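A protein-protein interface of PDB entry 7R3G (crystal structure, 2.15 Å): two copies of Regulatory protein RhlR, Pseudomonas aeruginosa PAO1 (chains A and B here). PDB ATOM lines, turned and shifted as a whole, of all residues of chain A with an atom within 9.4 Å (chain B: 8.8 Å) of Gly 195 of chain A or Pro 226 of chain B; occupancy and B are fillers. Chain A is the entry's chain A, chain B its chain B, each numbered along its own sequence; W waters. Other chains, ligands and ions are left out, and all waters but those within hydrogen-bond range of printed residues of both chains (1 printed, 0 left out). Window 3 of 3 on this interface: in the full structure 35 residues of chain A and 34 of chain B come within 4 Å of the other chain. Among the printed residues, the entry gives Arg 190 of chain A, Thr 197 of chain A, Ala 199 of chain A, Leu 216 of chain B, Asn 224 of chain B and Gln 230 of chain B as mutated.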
ATOM      1  N   ILE A 188     -25.133   3.025  -6.648  1.00  0.00           N
ATOM      2  CA  ILE A 188     -26.441   2.572  -6.181  1.00  0.00           C
ATOM      3  C   ILE A 188     -27.070   1.627  -7.199  1.00  0.00           C
ATOM      4  O   ILE A 188     -27.720   0.640  -6.835  1.00  0.00           O
ATOM      5  CB  ILE A 188     -27.352   3.779  -5.884  1.00  0.00           C
ATOM      6  CG1 ILE A 188     -27.010   4.366  -4.508  1.00  0.00           C
ATOM      7  CG2 ILE A 188     -28.822   3.370  -5.968  1.00  0.00           C
ATOM      8  CD1 ILE A 188     -27.689   5.689  -4.209  1.00  0.00           C
ATOM      9  N   LEU A 189     -26.893   1.915  -8.488  1.00  0.00           N
ATOM     10  CA  LEU A 189     -27.459   1.048  -9.516  1.00  0.00           C
ATOM     11  C   LEU A 189     -26.753  -0.303  -9.558  1.00  0.00           C
ATOM     12  O   LEU A 189     -27.392  -1.324  -9.839  1.00  0.00           O
ATOM     13  CB  LEU A 189     -27.380   1.740 -10.876  1.00  0.00           C
ATOM     14  CG  LEU A 189     -28.189   1.127 -12.018  1.00  0.00           C
ATOM     15  CD1 LEU A 189     -29.658   1.006 -11.638  1.00  0.00           C
ATOM     16  CD2 LEU A 189     -28.027   1.944 -13.304  1.00  0.00           C
ATOM     17  N   ARG A 190     -25.446  -0.329  -9.282  1.00  0.00           N
ATOM     18  CA  ARG A 190     -24.722  -1.595  -9.226  1.00  0.00           C
ATOM     19  C   ARG A 190     -25.301  -2.507  -8.153  1.00  0.00           C
ATOM     20  O   ARG A 190     -25.620  -3.672  -8.416  1.00  0.00           O
ATOM     21  CB  ARG A 190     -23.240  -1.348  -8.958  1.00  0.00           C
ATOM     22  CG  ARG A 190     -22.379  -1.327 -10.197  1.00  0.00           C
ATOM     23  CD  ARG A 190     -20.971  -0.843  -9.888  1.00  0.00           C
ATOM     24  NE  ARG A 190     -20.400  -0.133 -11.026  1.00  0.00           N
ATOM     25  CZ  ARG A 190     -19.203   0.439 -11.035  1.00  0.00           C
ATOM     26  NH1 ARG A 190     -18.411   0.407  -9.975  1.00  0.00           N
ATOM     27  NH2 ARG A 190     -18.790   1.057 -12.138  1.00  0.00           N
ATOM     28  N   TRP A 191     -25.421  -1.997  -6.923  1.00  0.00           N
ATOM     29  CA  TRP A 191     -26.039  -2.786  -5.864  1.00  0.00           C
ATOM     30  C   TRP A 191     -27.455  -3.195  -6.245  1.00  0.00           C
ATOM     31  O   TRP A 191     -27.875  -4.326  -5.979  1.00  0.00           O
ATOM     32  CB  TRP A 191     -26.060  -1.998  -4.553  1.00  0.00           C
ATOM     33  CG  TRP A 191     -24.725  -1.828  -3.911  1.00  0.00           C
ATOM     34  CD1 TRP A 191     -24.027  -0.665  -3.776  1.00  0.00           C
ATOM     35  CD2 TRP A 191     -23.923  -2.850  -3.304  1.00  0.00           C
ATOM     36  NE1 TRP A 191     -22.839  -0.898  -3.128  1.00  0.00           N
ATOM     37  CE2 TRP A 191     -22.752  -2.231  -2.826  1.00  0.00           C
ATOM     38  CE3 TRP A 191     -24.084  -4.227  -3.118  1.00  0.00           C
ATOM     39  CZ2 TRP A 191     -21.743  -2.941  -2.174  1.00  0.00           C
ATOM     40  CZ3 TRP A 191     -23.081  -4.932  -2.474  1.00  0.00           C
ATOM     41  CH2 TRP A 191     -21.925  -4.287  -2.009  1.00  0.00           C
ATOM     42  N   THR A 192     -28.211  -2.286  -6.862  1.00  0.00           N
ATOM     43  CA  THR A 192     -29.566  -2.622  -7.288  1.00  0.00           C
ATOM     44  C   THR A 192     -29.547  -3.772  -8.284  1.00  0.00           C
ATOM     45  O   THR A 192     -30.288  -4.751  -8.136  1.00  0.00           O
ATOM     46  CB  THR A 192     -30.241  -1.390  -7.893  1.00  0.00           C
ATOM     47  OG1 THR A 192     -30.410  -0.397  -6.873  1.00  0.00           O
ATOM     48  CG2 THR A 192     -31.594  -1.754  -8.485  1.00  0.00           C
ATOM     49  N   ALA A 193     -28.693  -3.674  -9.304  1.00  0.00           N
ATOM     50  CA  ALA A 193     -28.585  -4.749 -10.281  1.00  0.00           C
ATOM     51  C   ALA A 193     -28.124  -6.050  -9.642  1.00  0.00           C
ATOM     52  O   ALA A 193     -28.379  -7.124 -10.199  1.00  0.00           O
ATOM     53  CB  ALA A 193     -27.626  -4.349 -11.401  1.00  0.00           C
ATOM     54  N   ASP A 194     -27.454  -5.981  -8.491  1.00  0.00           N
ATOM     55  CA  ASP A 194     -27.069  -7.166  -7.740  1.00  0.00           C
ATOM     56  C   ASP A 194     -28.159  -7.627  -6.778  1.00  0.00           C
ATOM     57  O   ASP A 194     -27.897  -8.487  -5.932  1.00  0.00           O
ATOM     58  CB  ASP A 194     -25.775  -6.909  -6.961  1.00  0.00           C
ATOM     59  CG  ASP A 194     -24.530  -7.073  -7.816  1.00  0.00           C
ATOM     60  OD1 ASP A 194     -24.598  -7.736  -8.874  1.00  0.00           O
ATOM     61  OD2 ASP A 194     -23.473  -6.536  -7.422  1.00  0.00           O
ATOM     62  N   GLY A 195     -29.360  -7.064  -6.873  1.00  0.00           N
ATOM     63  CA  GLY A 195     -30.503  -7.564  -6.136  1.00  0.00           C
ATOM     64  C   GLY A 195     -30.714  -6.991  -4.755  1.00  0.00           C
ATOM     65  O   GLY A 195     -31.542  -7.524  -4.007  1.00  0.00           O
ATOM     66  N   LYS A 196     -30.004  -5.928  -4.390  1.00  0.00           N
ATOM     67  CA  LYS A 196     -30.186  -5.314  -3.084  1.00  0.00           C
ATOM     68  C   LYS A 196     -31.393  -4.379  -3.084  1.00  0.00           C
ATOM     69  O   LYS A 196     -31.710  -3.731  -4.087  1.00  0.00           O
ATOM     70  CB  LYS A 196     -28.931  -4.540  -2.680  1.00  0.00           C
ATOM     71  CG  LYS A 196     -27.666  -5.384  -2.634  1.00  0.00           C
ATOM     72  CD  LYS A 196     -27.742  -6.446  -1.549  1.00  0.00           C
ATOM     73  CE  LYS A 196     -26.397  -7.133  -1.341  1.00  0.00           C
ATOM     74  NZ  LYS A 196     -26.269  -7.688   0.036  1.00  0.00           N
ATOM     75  N   THR A 197     -32.067  -4.317  -1.940  1.00  0.00           N
ATOM     76  CA  THR A 197     -33.173  -3.393  -1.752  1.00  0.00           C
ATOM     77  C   THR A 197     -32.647  -2.018  -1.347  1.00  0.00           C
ATOM     78  O   THR A 197     -31.462  -1.835  -1.047  1.00  0.00           O
ATOM     79  CB  THR A 197     -34.140  -3.921  -0.694  1.00  0.00           C
ATOM     80  OG1 THR A 197     -33.470  -3.995   0.570  1.00  0.00           O
ATOM     81  CG2 THR A 197     -34.648  -5.301  -1.074  1.00  0.00           C
ATOM     82  N   SER A 198     -33.545  -1.031  -1.353  1.00  0.00           N
ATOM     83  CA  SER A 198     -33.155   0.299  -0.901  1.00  0.00           C
ATOM     84  C   SER A 198     -32.628   0.252   0.527  1.00  0.00           C
ATOM     85  O   SER A 198     -31.631   0.907   0.853  1.00  0.00           O
ATOM     86  CB  SER A 198     -34.336   1.263  -1.000  1.00  0.00           C
ATOM     87  OG  SER A 198     -34.731   1.434  -2.346  1.00  0.00           O
ATOM     88  N   ALA A 199     -33.281  -0.528   1.391  1.00  0.00           N
ATOM     89  CA  ALA A 199     -32.868  -0.595   2.789  1.00  0.00           C
ATOM     90  C   ALA A 199     -31.457  -1.157   2.913  1.00  0.00           C
ATOM     91  O   ALA A 199     -30.619  -0.608   3.638  1.00  0.00           O
ATOM     92  CB  ALA A 199     -33.861  -1.441   3.588  1.00  0.00           C
ATOM     93  N   GLU A 200     -31.172  -2.254   2.206  1.00  0.00           N
ATOM     94  CA  GLU A 200     -29.830  -2.824   2.252  1.00  0.00           C
ATOM     95  C   GLU A 200     -28.801  -1.835   1.719  1.00  0.00           C
ATOM     96  O   GLU A 200     -27.743  -1.636   2.329  1.00  0.00           O
ATOM     97  CB  GLU A 200     -29.788  -4.134   1.463  1.00  0.00           C
ATOM     98  CG  GLU A 200     -30.780  -5.186   1.958  1.00  0.00           C
ATOM     99  CD  GLU A 200     -30.775  -6.457   1.122  1.00  0.00           C
ATOM    100  OE1 GLU A 200     -31.132  -6.391  -0.074  1.00  0.00           O
ATOM    101  OE2 GLU A 200     -30.423  -7.526   1.666  1.00  0.00           O
ATOM    102  N   ILE A 201     -29.100  -1.194   0.587  1.00  0.00           N
ATOM    103  CA  ILE A 201     -28.170  -0.226   0.010  1.00  0.00           C
ATOM    104  C   ILE A 201     -27.941   0.925   0.980  1.00  0.00           C
ATOM    105  O   ILE A 201     -26.815   1.414   1.131  1.00  0.00           O
ATOM    106  CB  ILE A 201     -28.698   0.275  -1.350  1.00  0.00           C
ATOM    107  CG1 ILE A 201     -28.773  -0.879  -2.359  1.00  0.00           C
ATOM    108  CG2 ILE A 201     -27.816   1.393  -1.889  1.00  0.00           C
ATOM    109  CD1 ILE A 201     -29.530  -0.540  -3.658  1.00  0.00           C
ATOM    110  N   ILE A 204     -25.492  -0.243   3.478  1.00  0.00           N
ATOM    111  CA  ILE A 204     -24.161  -0.438   2.907  1.00  0.00           C
ATOM    112  C   ILE A 204     -23.444   0.896   2.748  1.00  0.00           C
ATOM    113  O   ILE A 204     -22.254   1.021   3.065  1.00  0.00           O
ATOM    114  CB  ILE A 204     -24.249  -1.182   1.563  1.00  0.00           C
ATOM    115  CG1 ILE A 204     -24.538  -2.664   1.796  1.00  0.00           C
ATOM    116  CG2 ILE A 204     -22.955  -0.979   0.765  1.00  0.00           C
ATOM    117  CD1 ILE A 204     -24.855  -3.424   0.525  1.00  0.00           C
ATOM    118  N   LYS A 228     -37.113   0.359 -11.902  1.00  0.00           N
ATOM    119  CA  LYS A 228     -35.678   0.158 -11.741  1.00  0.00           C
ATOM    120  C   LYS A 228     -35.187  -1.082 -12.477  1.00  0.00           C
ATOM    121  O   LYS A 228     -33.984  -1.197 -12.738  1.00  0.00           O
ATOM    122  CB  LYS A 228     -35.322   0.081 -10.251  1.00  0.00           C
ATOM    123  CG  LYS A 228     -35.839  -1.152  -9.522  1.00  0.00           C
ATOM    124  CD  LYS A 228     -36.037  -0.884  -8.028  1.00  0.00           C
ATOM    125  CE  LYS A 228     -35.271  -1.885  -7.165  1.00  0.00           C
ATOM    126  NZ  LYS A 228     -35.512  -1.678  -5.704  1.00  0.00           N
ATOM    127  N   ALA A 232     -31.677  -0.904 -14.575  1.00  0.00           N
ATOM    128  CA  ALA A 232     -30.535  -1.762 -14.270  1.00  0.00           C
ATOM    129  C   ALA A 232     -30.159  -2.628 -15.465  1.00  0.00           C
ATOM    130  O   ALA A 232     -28.972  -2.827 -15.743  1.00  0.00           O
ATOM    131  CB  ALA A 232     -30.839  -2.638 -13.056  1.00  0.00           C
ATOM    132  N   ILE A 241     -22.540  -0.133 -15.794  1.00  0.00           N
ATOM    133  CA  ILE A 241     -22.287  -0.624 -14.443  1.00  0.00           C
ATOM    134  C   ILE A 241     -21.368  -1.838 -14.528  1.00  0.00           C
ATOM    135  O   ILE A 241     -20.607  -2.139 -13.606  1.00  0.00           O
ATOM    136  CB  ILE A 241     -23.587  -0.978 -13.713  1.00  0.00           C
ATOM    137  CG1 ILE A 241     -24.503  -1.794 -14.625  1.00  0.00           C
ATOM    138  CG2 ILE A 241     -24.301   0.282 -13.246  1.00  0.00           C
ATOM    139  CD1 ILE A 241     -25.577  -2.543 -13.886  1.00  0.00           C
ATOM    140  OXT ILE A 241     -21.379  -2.551 -15.534  1.00  0.00           O
ATOM    141  N   PRO B  52     -20.640 -10.705 -10.284  1.00  0.00           N
ATOM    142  CA  PRO B  52     -21.549  -9.687  -9.727  1.00  0.00           C
ATOM    143  C   PRO B  52     -21.050  -8.271 -10.007  1.00  0.00           C
ATOM    144  O   PRO B  52     -19.838  -8.054 -10.029  1.00  0.00           O
ATOM    145  CB  PRO B  52     -21.539  -9.980  -8.222  1.00  0.00           C
ATOM    146  CG  PRO B  52     -21.050 -11.395  -8.098  1.00  0.00           C
ATOM    147  CD  PRO B  52     -20.090 -11.585  -9.236  1.00  0.00           C
ATOM    148  N   PHE B  53     -21.965  -7.328 -10.234  1.00  0.00           N
ATOM    149  CA  PHE B  53     -21.547  -6.001 -10.679  1.00  0.00           C
ATOM    150  C   PHE B  53     -20.639  -5.336  -9.650  1.00  0.00           C
ATOM    151  O   PHE B  53     -19.693  -4.627 -10.009  1.00  0.00           O
ATOM    152  CB  PHE B  53     -22.769  -5.125 -10.967  1.00  0.00           C
ATOM    153  CG  PHE B  53     -23.599  -5.598 -12.135  1.00  0.00           C
ATOM    154  CD1 PHE B  53     -23.147  -5.446 -13.437  1.00  0.00           C
ATOM    155  CD2 PHE B  53     -24.836  -6.190 -11.929  1.00  0.00           C
ATOM    156  CE1 PHE B  53     -23.911  -5.879 -14.511  1.00  0.00           C
ATOM    157  CE2 PHE B  53     -25.606  -6.626 -13.002  1.00  0.00           C
ATOM    158  CZ  PHE B  53     -25.142  -6.468 -14.291  1.00  0.00           C
ATOM    159  N   THR B  54     -20.908  -5.552  -8.362  1.00  0.00           N
ATOM    160  CA  THR B  54     -20.144  -4.872  -7.323  1.00  0.00           C
ATOM    161  C   THR B  54     -18.824  -5.570  -7.011  1.00  0.00           C
ATOM    162  O   THR B  54     -17.908  -4.925  -6.486  1.00  0.00           O
ATOM    163  CB  THR B  54     -20.978  -4.757  -6.044  1.00  0.00           C
ATOM    164  OG1 THR B  54     -21.340  -6.065  -5.583  1.00  0.00           O
ATOM    165  CG2 THR B  54     -22.248  -3.944  -6.297  1.00  0.00           C
ATOM    166  N   LEU B 216     -41.205 -16.343 -13.956  1.00  0.00           N
ATOM    167  CA  LEU B 216     -40.270 -15.408 -13.340  1.00  0.00           C
ATOM    168  C   LEU B 216     -39.693 -15.977 -12.049  1.00  0.00           C
ATOM    169  O   LEU B 216     -38.500 -15.814 -11.768  1.00  0.00           O
ATOM    170  CB  LEU B 216     -40.963 -14.072 -13.084  1.00  0.00           C
ATOM    171  CG  LEU B 216     -41.085 -13.175 -14.316  1.00  0.00           C
ATOM    172  CD1 LEU B 216     -41.953 -11.965 -14.024  1.00  0.00           C
ATOM    173  CD2 LEU B 216     -39.711 -12.739 -14.811  1.00  0.00           C
ATOM    174  N   LYS B 217     -40.521 -16.653 -11.253  1.00  0.00           N
ATOM    175  CA  LYS B 217     -40.005 -17.319 -10.061  1.00  0.00           C
ATOM    176  C   LYS B 217     -38.985 -18.392 -10.434  1.00  0.00           C
ATOM    177  O   LYS B 217     -38.002 -18.605  -9.715  1.00  0.00           O
ATOM    178  CB  LYS B 217     -41.155 -17.914  -9.250  1.00  0.00           C
ATOM    179  CG  LYS B 217     -41.828 -16.910  -8.321  1.00  0.00           C
ATOM    180  CD  LYS B 217     -42.978 -17.542  -7.556  1.00  0.00           C
ATOM    181  CE  LYS B 217     -44.185 -16.618  -7.504  1.00  0.00           C
ATOM    182  NZ  LYS B 217     -44.726 -16.505  -6.120  1.00  0.00           N
ATOM    183  N   ILE B 219     -37.117 -18.384 -13.395  1.00  0.00           N
ATOM    184  CA  ILE B 219     -35.964 -17.631 -13.886  1.00  0.00           C
ATOM    185  C   ILE B 219     -35.129 -17.131 -12.713  1.00  0.00           C
ATOM    186  O   ILE B 219     -33.899 -17.254 -12.697  1.00  0.00           O
ATOM    187  CB  ILE B 219     -36.428 -16.467 -14.779  1.00  0.00           C
ATOM    188  CG1 ILE B 219     -37.054 -17.006 -16.068  1.00  0.00           C
ATOM    189  CG2 ILE B 219     -35.269 -15.523 -15.088  1.00  0.00           C
ATOM    190  CD1 ILE B 219     -37.801 -15.958 -16.871  1.00  0.00           C
ATOM    191  N   GLN B 220     -35.795 -16.565 -11.706  1.00  0.00           N
ATOM    192  CA  GLN B 220     -35.071 -16.037 -10.556  1.00  0.00           C
ATOM    193  C   GLN B 220     -34.307 -17.137  -9.836  1.00  0.00           C
ATOM    194  O   GLN B 220     -33.170 -16.927  -9.395  1.00  0.00           O
ATOM    195  CB  GLN B 220     -36.046 -15.329  -9.620  1.00  0.00           C
ATOM    196  CG  GLN B 220     -36.458 -13.970 -10.157  1.00  0.00           C
ATOM    197  CD  GLN B 220     -37.656 -13.385  -9.452  1.00  0.00           C
ATOM    198  OE1 GLN B 220     -38.539 -12.813 -10.088  1.00  0.00           O
ATOM    199  NE2 GLN B 220     -37.692 -13.514  -8.131  1.00  0.00           N
ATOM    200  N   LYS B 221     -34.904 -18.326  -9.724  1.00  0.00           N
ATOM    201  CA  LYS B 221     -34.195 -19.445  -9.112  1.00  0.00           C
ATOM    202  C   LYS B 221     -32.949 -19.805  -9.913  1.00  0.00           C
ATOM    203  O   LYS B 221     -31.890 -20.079  -9.338  1.00  0.00           O
ATOM    204  CB  LYS B 221     -35.125 -20.653  -8.991  1.00  0.00           C
ATOM    205  N   PHE B 223     -31.084 -17.880 -11.676  1.00  0.00           N
ATOM    206  CA  PHE B 223     -30.077 -16.870 -11.391  1.00  0.00           C
ATOM    207  C   PHE B 223     -29.734 -16.790  -9.909  1.00  0.00           C
ATOM    208  O   PHE B 223     -28.911 -15.952  -9.524  1.00  0.00           O
ATOM    209  CB  PHE B 223     -30.555 -15.497 -11.879  1.00  0.00           C
ATOM    210  CG  PHE B 223     -30.421 -15.298 -13.365  1.00  0.00           C
ATOM    211  CD1 PHE B 223     -29.183 -15.053 -13.936  1.00  0.00           C
ATOM    212  CD2 PHE B 223     -31.534 -15.352 -14.189  1.00  0.00           C
ATOM    213  CE1 PHE B 223     -29.057 -14.867 -15.303  1.00  0.00           C
ATOM    214  CE2 PHE B 223     -31.415 -15.169 -15.558  1.00  0.00           C
ATOM    215  CZ  PHE B 223     -30.174 -14.924 -16.114  1.00  0.00           C
ATOM    216  N   ASN B 224     -30.330 -17.639  -9.075  1.00  0.00           N
ATOM    217  CA  ASN B 224     -30.191 -17.528  -7.627  1.00  0.00           C
ATOM    218  C   ASN B 224     -30.378 -16.074  -7.195  1.00  0.00           C
ATOM    219  O   ASN B 224     -29.573 -15.504  -6.455  1.00  0.00           O
ATOM    220  CB  ASN B 224     -28.840 -18.071  -7.164  1.00  0.00           C
ATOM    221  CG  ASN B 224     -28.726 -18.137  -5.656  1.00  0.00           C
ATOM    222  OD1 ASN B 224     -27.808 -17.566  -5.067  1.00  0.00           O
ATOM    223  ND2 ASN B 224     -29.662 -18.834  -5.019  1.00  0.00           N
ATOM    224  N   ALA B 225     -31.462 -15.464  -7.690  1.00  0.00           N
ATOM    225  CA  ALA B 225     -31.706 -14.042  -7.527  1.00  0.00           C
ATOM    226  C   ALA B 225     -32.928 -13.795  -6.654  1.00  0.00           C
ATOM    227  O   ALA B 225     -33.935 -14.499  -6.784  1.00  0.00           O
ATOM    228  CB  ALA B 225     -31.915 -13.372  -8.892  1.00  0.00           C
ATOM    229  N   PRO B 226     -32.875 -12.798  -5.762  1.00  0.00           N
ATOM    230  CA  PRO B 226     -34.033 -12.539  -4.891  1.00  0.00           C
ATOM    231  C   PRO B 226     -35.148 -11.753  -5.556  1.00  0.00           C
ATOM    232  O   PRO B 226     -36.264 -11.736  -5.021  1.00  0.00           O
ATOM    233  CB  PRO B 226     -33.425 -11.742  -3.729  1.00  0.00           C
ATOM    234  CG  PRO B 226     -32.271 -11.010  -4.358  1.00  0.00           C
ATOM    235  CD  PRO B 226     -31.754 -11.876  -5.490  1.00  0.00           C
ATOM    236  N   ASN B 227     -34.891 -11.095  -6.685  1.00  0.00           N
ATOM    237  CA  ASN B 227     -35.927 -10.347  -7.383  1.00  0.00           C
ATOM    238  C   ASN B 227     -35.678 -10.437  -8.883  1.00  0.00           C
ATOM    239  O   ASN B 227     -34.690 -11.019  -9.340  1.00  0.00           O
ATOM    240  CB  ASN B 227     -35.977  -8.886  -6.923  1.00  0.00           C
ATOM    241  CG  ASN B 227     -34.607  -8.246  -6.864  1.00  0.00           C
ATOM    242  OD1 ASN B 227     -34.067  -7.808  -7.880  1.00  0.00           O
ATOM    243  ND2 ASN B 227     -34.038  -8.183  -5.667  1.00  0.00           N
ATOM    244  N   LYS B 228     -36.592  -9.845  -9.654  1.00  0.00           N
ATOM    245  CA  LYS B 228     -36.472  -9.867 -11.105  1.00  0.00           C
ATOM    246  C   LYS B 228     -35.507  -8.812 -11.624  1.00  0.00           C
ATOM    247  O   LYS B 228     -35.028  -8.933 -12.757  1.00  0.00           O
ATOM    248  CB  LYS B 228     -37.843  -9.657 -11.753  1.00  0.00           C
ATOM    249  CG  LYS B 228     -38.462  -8.300 -11.451  1.00  0.00           C
ATOM    250  CD  LYS B 228     -39.667  -8.018 -12.333  1.00  0.00           C
ATOM    251  CE  LYS B 228     -40.953  -8.476 -11.670  1.00  0.00           C
ATOM    252  NZ  LYS B 228     -42.102  -8.475 -12.618  1.00  0.00           N
ATOM    253  N   THR B 229     -35.234  -7.770 -10.838  1.00  0.00           N
ATOM    254  CA  THR B 229     -34.263  -6.769 -11.259  1.00  0.00           C
ATOM    255  C   THR B 229     -32.891  -7.400 -11.452  1.00  0.00           C
ATOM    256  O   THR B 229     -32.210  -7.141 -12.452  1.00  0.00           O
ATOM    257  CB  THR B 229     -34.194  -5.635 -10.238  1.00  0.00           C
ATOM    258  OG1 THR B 229     -35.465  -4.976 -10.161  1.00  0.00           O
ATOM    259  CG2 THR B 229     -33.116  -4.629 -10.635  1.00  0.00           C
ATOM    260  N   GLN B 230     -32.467  -8.245 -10.506  1.00  0.00           N
ATOM    261  CA  GLN B 230     -31.172  -8.902 -10.645  1.00  0.00           C
ATOM    262  C   GLN B 230     -31.177  -9.891 -11.803  1.00  0.00           C
ATOM    263  O   GLN B 230     -30.211  -9.959 -12.571  1.00  0.00           O
ATOM    264  CB  GLN B 230     -30.781  -9.622  -9.356  1.00  0.00           C
ATOM    265  CG  GLN B 230     -29.381 -10.239  -9.417  1.00  0.00           C
ATOM    266  CD  GLN B 230     -29.076 -11.122  -8.225  1.00  0.00           C
ATOM    267  OE1 GLN B 230     -29.417 -10.789  -7.091  1.00  0.00           O
ATOM    268  NE2 GLN B 230     -28.429 -12.253  -8.474  1.00  0.00           N
ATOM    269  N   ALA B 231     -32.239 -10.689 -11.926  1.00  0.00           N
ATOM    270  CA  ALA B 231     -32.321 -11.638 -13.030  1.00  0.00           C
ATOM    271  C   ALA B 231     -32.183 -10.931 -14.373  1.00  0.00           C
ATOM    272  O   ALA B 231     -31.472 -11.407 -15.266  1.00  0.00           O
ATOM    273  CB  ALA B 231     -33.643 -12.403 -12.961  1.00  0.00           C
ATOM    274  N   ALA B 233     -30.855  -7.835 -15.073  1.00  0.00           N
ATOM    275  CA  ALA B 233     -29.553  -7.212 -15.272  1.00  0.00           C
ATOM    276  C   ALA B 233     -28.477  -8.261 -15.512  1.00  0.00           C
ATOM    277  O   ALA B 233     -27.587  -8.066 -16.349  1.00  0.00           O
ATOM    278  CB  ALA B 233     -29.201  -6.346 -14.065  1.00  0.00           C
ATOM    279  N   TYR B 234     -28.546  -9.383 -14.792  1.00  0.00           N
ATOM    280  CA  TYR B 234     -27.601 -10.468 -15.024  1.00  0.00           C
ATOM    281  C   TYR B 234     -27.776 -11.050 -16.420  1.00  0.00           C
ATOM    282  O   TYR B 234     -26.791 -11.302 -17.122  1.00  0.00           O
ATOM    283  CB  TYR B 234     -27.778 -11.547 -13.955  1.00  0.00           C
ATOM    284  CG  TYR B 234     -27.063 -11.243 -12.656  1.00  0.00           C
ATOM    285  CD1 TYR B 234     -26.811  -9.933 -12.266  1.00  0.00           C
ATOM    286  CD2 TYR B 234     -26.633 -12.266 -11.824  1.00  0.00           C
ATOM    287  CE1 TYR B 234     -26.151  -9.650 -11.085  1.00  0.00           C
ATOM    288  CE2 TYR B 234     -25.975 -11.993 -10.639  1.00  0.00           C
ATOM    289  CZ  TYR B 234     -25.737 -10.684 -10.273  1.00  0.00           C
ATOM    290  OH  TYR B 234     -25.083 -10.405  -9.100  1.00  0.00           O
HETATM  291  O   HOH W   1     -28.429 -11.563  -4.799  1.00  0.00           O
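Water W1 lies within hydrogen-bond range of the side-chain amide oxygen of Gln 230 of chain B (2.6 Å) and the backbone carbonyl oxygen of Asp 194 of chain A (3.3 Å).
The chain-end carboxylate of Ile 241 of chain A lies within salt-bridge range of the guanidinium group of Arg 190 of chain A, 3.3 Å away. The backbone carbonyl oxygen (O) of Ile 188 of chain A sits at hydrogen-bond distance from the side-chain hydroxyl (OG1) of Thr 192 of chain A, 2.9 Å away. The backbone NH of Thr 229 of chain B lies within hydrogen-bond range of the side-chain amide oxygen of Asn 227 of chain B (3.2 Å). The side-chain amide oxygen of Asn 227 of chain B is in hydrogen-bond range of the backbone NH of Gln 230 of chain B. The backbone carbonyl oxygen (O) of Trp 191 of chain A sits at hydrogen-bond distance from the backbone NH (N) of Lys 196 of chain A (3.1 Å).
CG2 of Thr 54 of chain B touches CB of Arg 190 of chain A, at 3.8 Å. CG2 of Thr 54 of chain B touches CD2 of Trp 191 of chain A, 3.6 Å away. CG2 of Thr 229 of chain B touches O of Thr 192 of chain A, at 3.8 Å. Gln 230 of chain B touches Ala 193 of chain A. Ala 193 of chain A touches Ala 233 of chain B (CB to CB, 3.7 Å). Ala 193 of chain A touches Tyr 234 of chain B. Pro 52 of chain B touches Asp 194 of chain A. Thr 229 of chain B touches Lys 228 of chain A (OG1 to CG, 3.9 Å). Ala 232 of chain A touches Ala 233 of chain B (O to CB, 3.9 Å). Ile 241 of chain A touches Phe 53 of chain B.
Gly 195 of chain A touches just these residues of chain B: Pro 226, Asn 227 and Gln 230. Of chain A, only Gly 195 comes within 4 Å of Pro 226 of chain B. Of chain A, only Gly 195 (3.1 Å) comes within 4 Å of Asn 227 of chain B. Printed residues of chain B within 4 Å of Arg 190 of chain A: Phe 53 (3.9 Å) and Thr 54 (3.8 Å). Printed residues of chain B within 4 Å of Ile 241 of chain A: Phe 53. Printed residues of chain B within 4 Å of Asp 194 of chain A: Pro 52 (3.7 Å), Phe 53 (3.0 Å), Thr 54 (2.9 Å), Gln 230 (3.0 Å) and Tyr 234 (2.7 Å). Of the printed residues of chain A, Thr 54 of chain B touches Arg 190 (3.8 Å), Trp 191 (3.6 Å) and Asp 194 (2.9 Å). Of the printed residues of chain A, Pro 52 of chain B touches Asp 194 (3.7 Å). The nearest printed residue of chain A that does not touch Thr 229 of chain B is Ala 193 of chain A (4.4 Å).
1 position is printed for both chains. Of the 20 pairs that touch across the chains among the printed residues, none has its exchanged pair printed and touching as well.
Of the 18 printed residues of chain A, 9 touch a printed residue of chain B. Among the printed residues, 20 pairs touch across the chains. Among the printed residues, no Asp or Glu carboxylate lies within 4 Å of a Lys or Arg side-chain nitrogen of the other chain.
OE1 of Gln 230 of chain B lies close to O of Asp 194 of chain A. OD1 of Asp 194 of chain A is in hydrogen-bond range of N of Phe 53 of chain B (3.0 Å). OH of Tyr 234 of chain B is in hydrogen-bond range of OD1 of Asp 194 of chain A. The side-chain carboxylate of Asp 194 of chain A is in hydrogen-bond range of the side-chain hydroxyl of Thr 54 of chain B (2.9 Å). ND2 of Asn 227 of chain B is in hydrogen-bond range of O of Gly 195 of chain A (3.1 Å).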
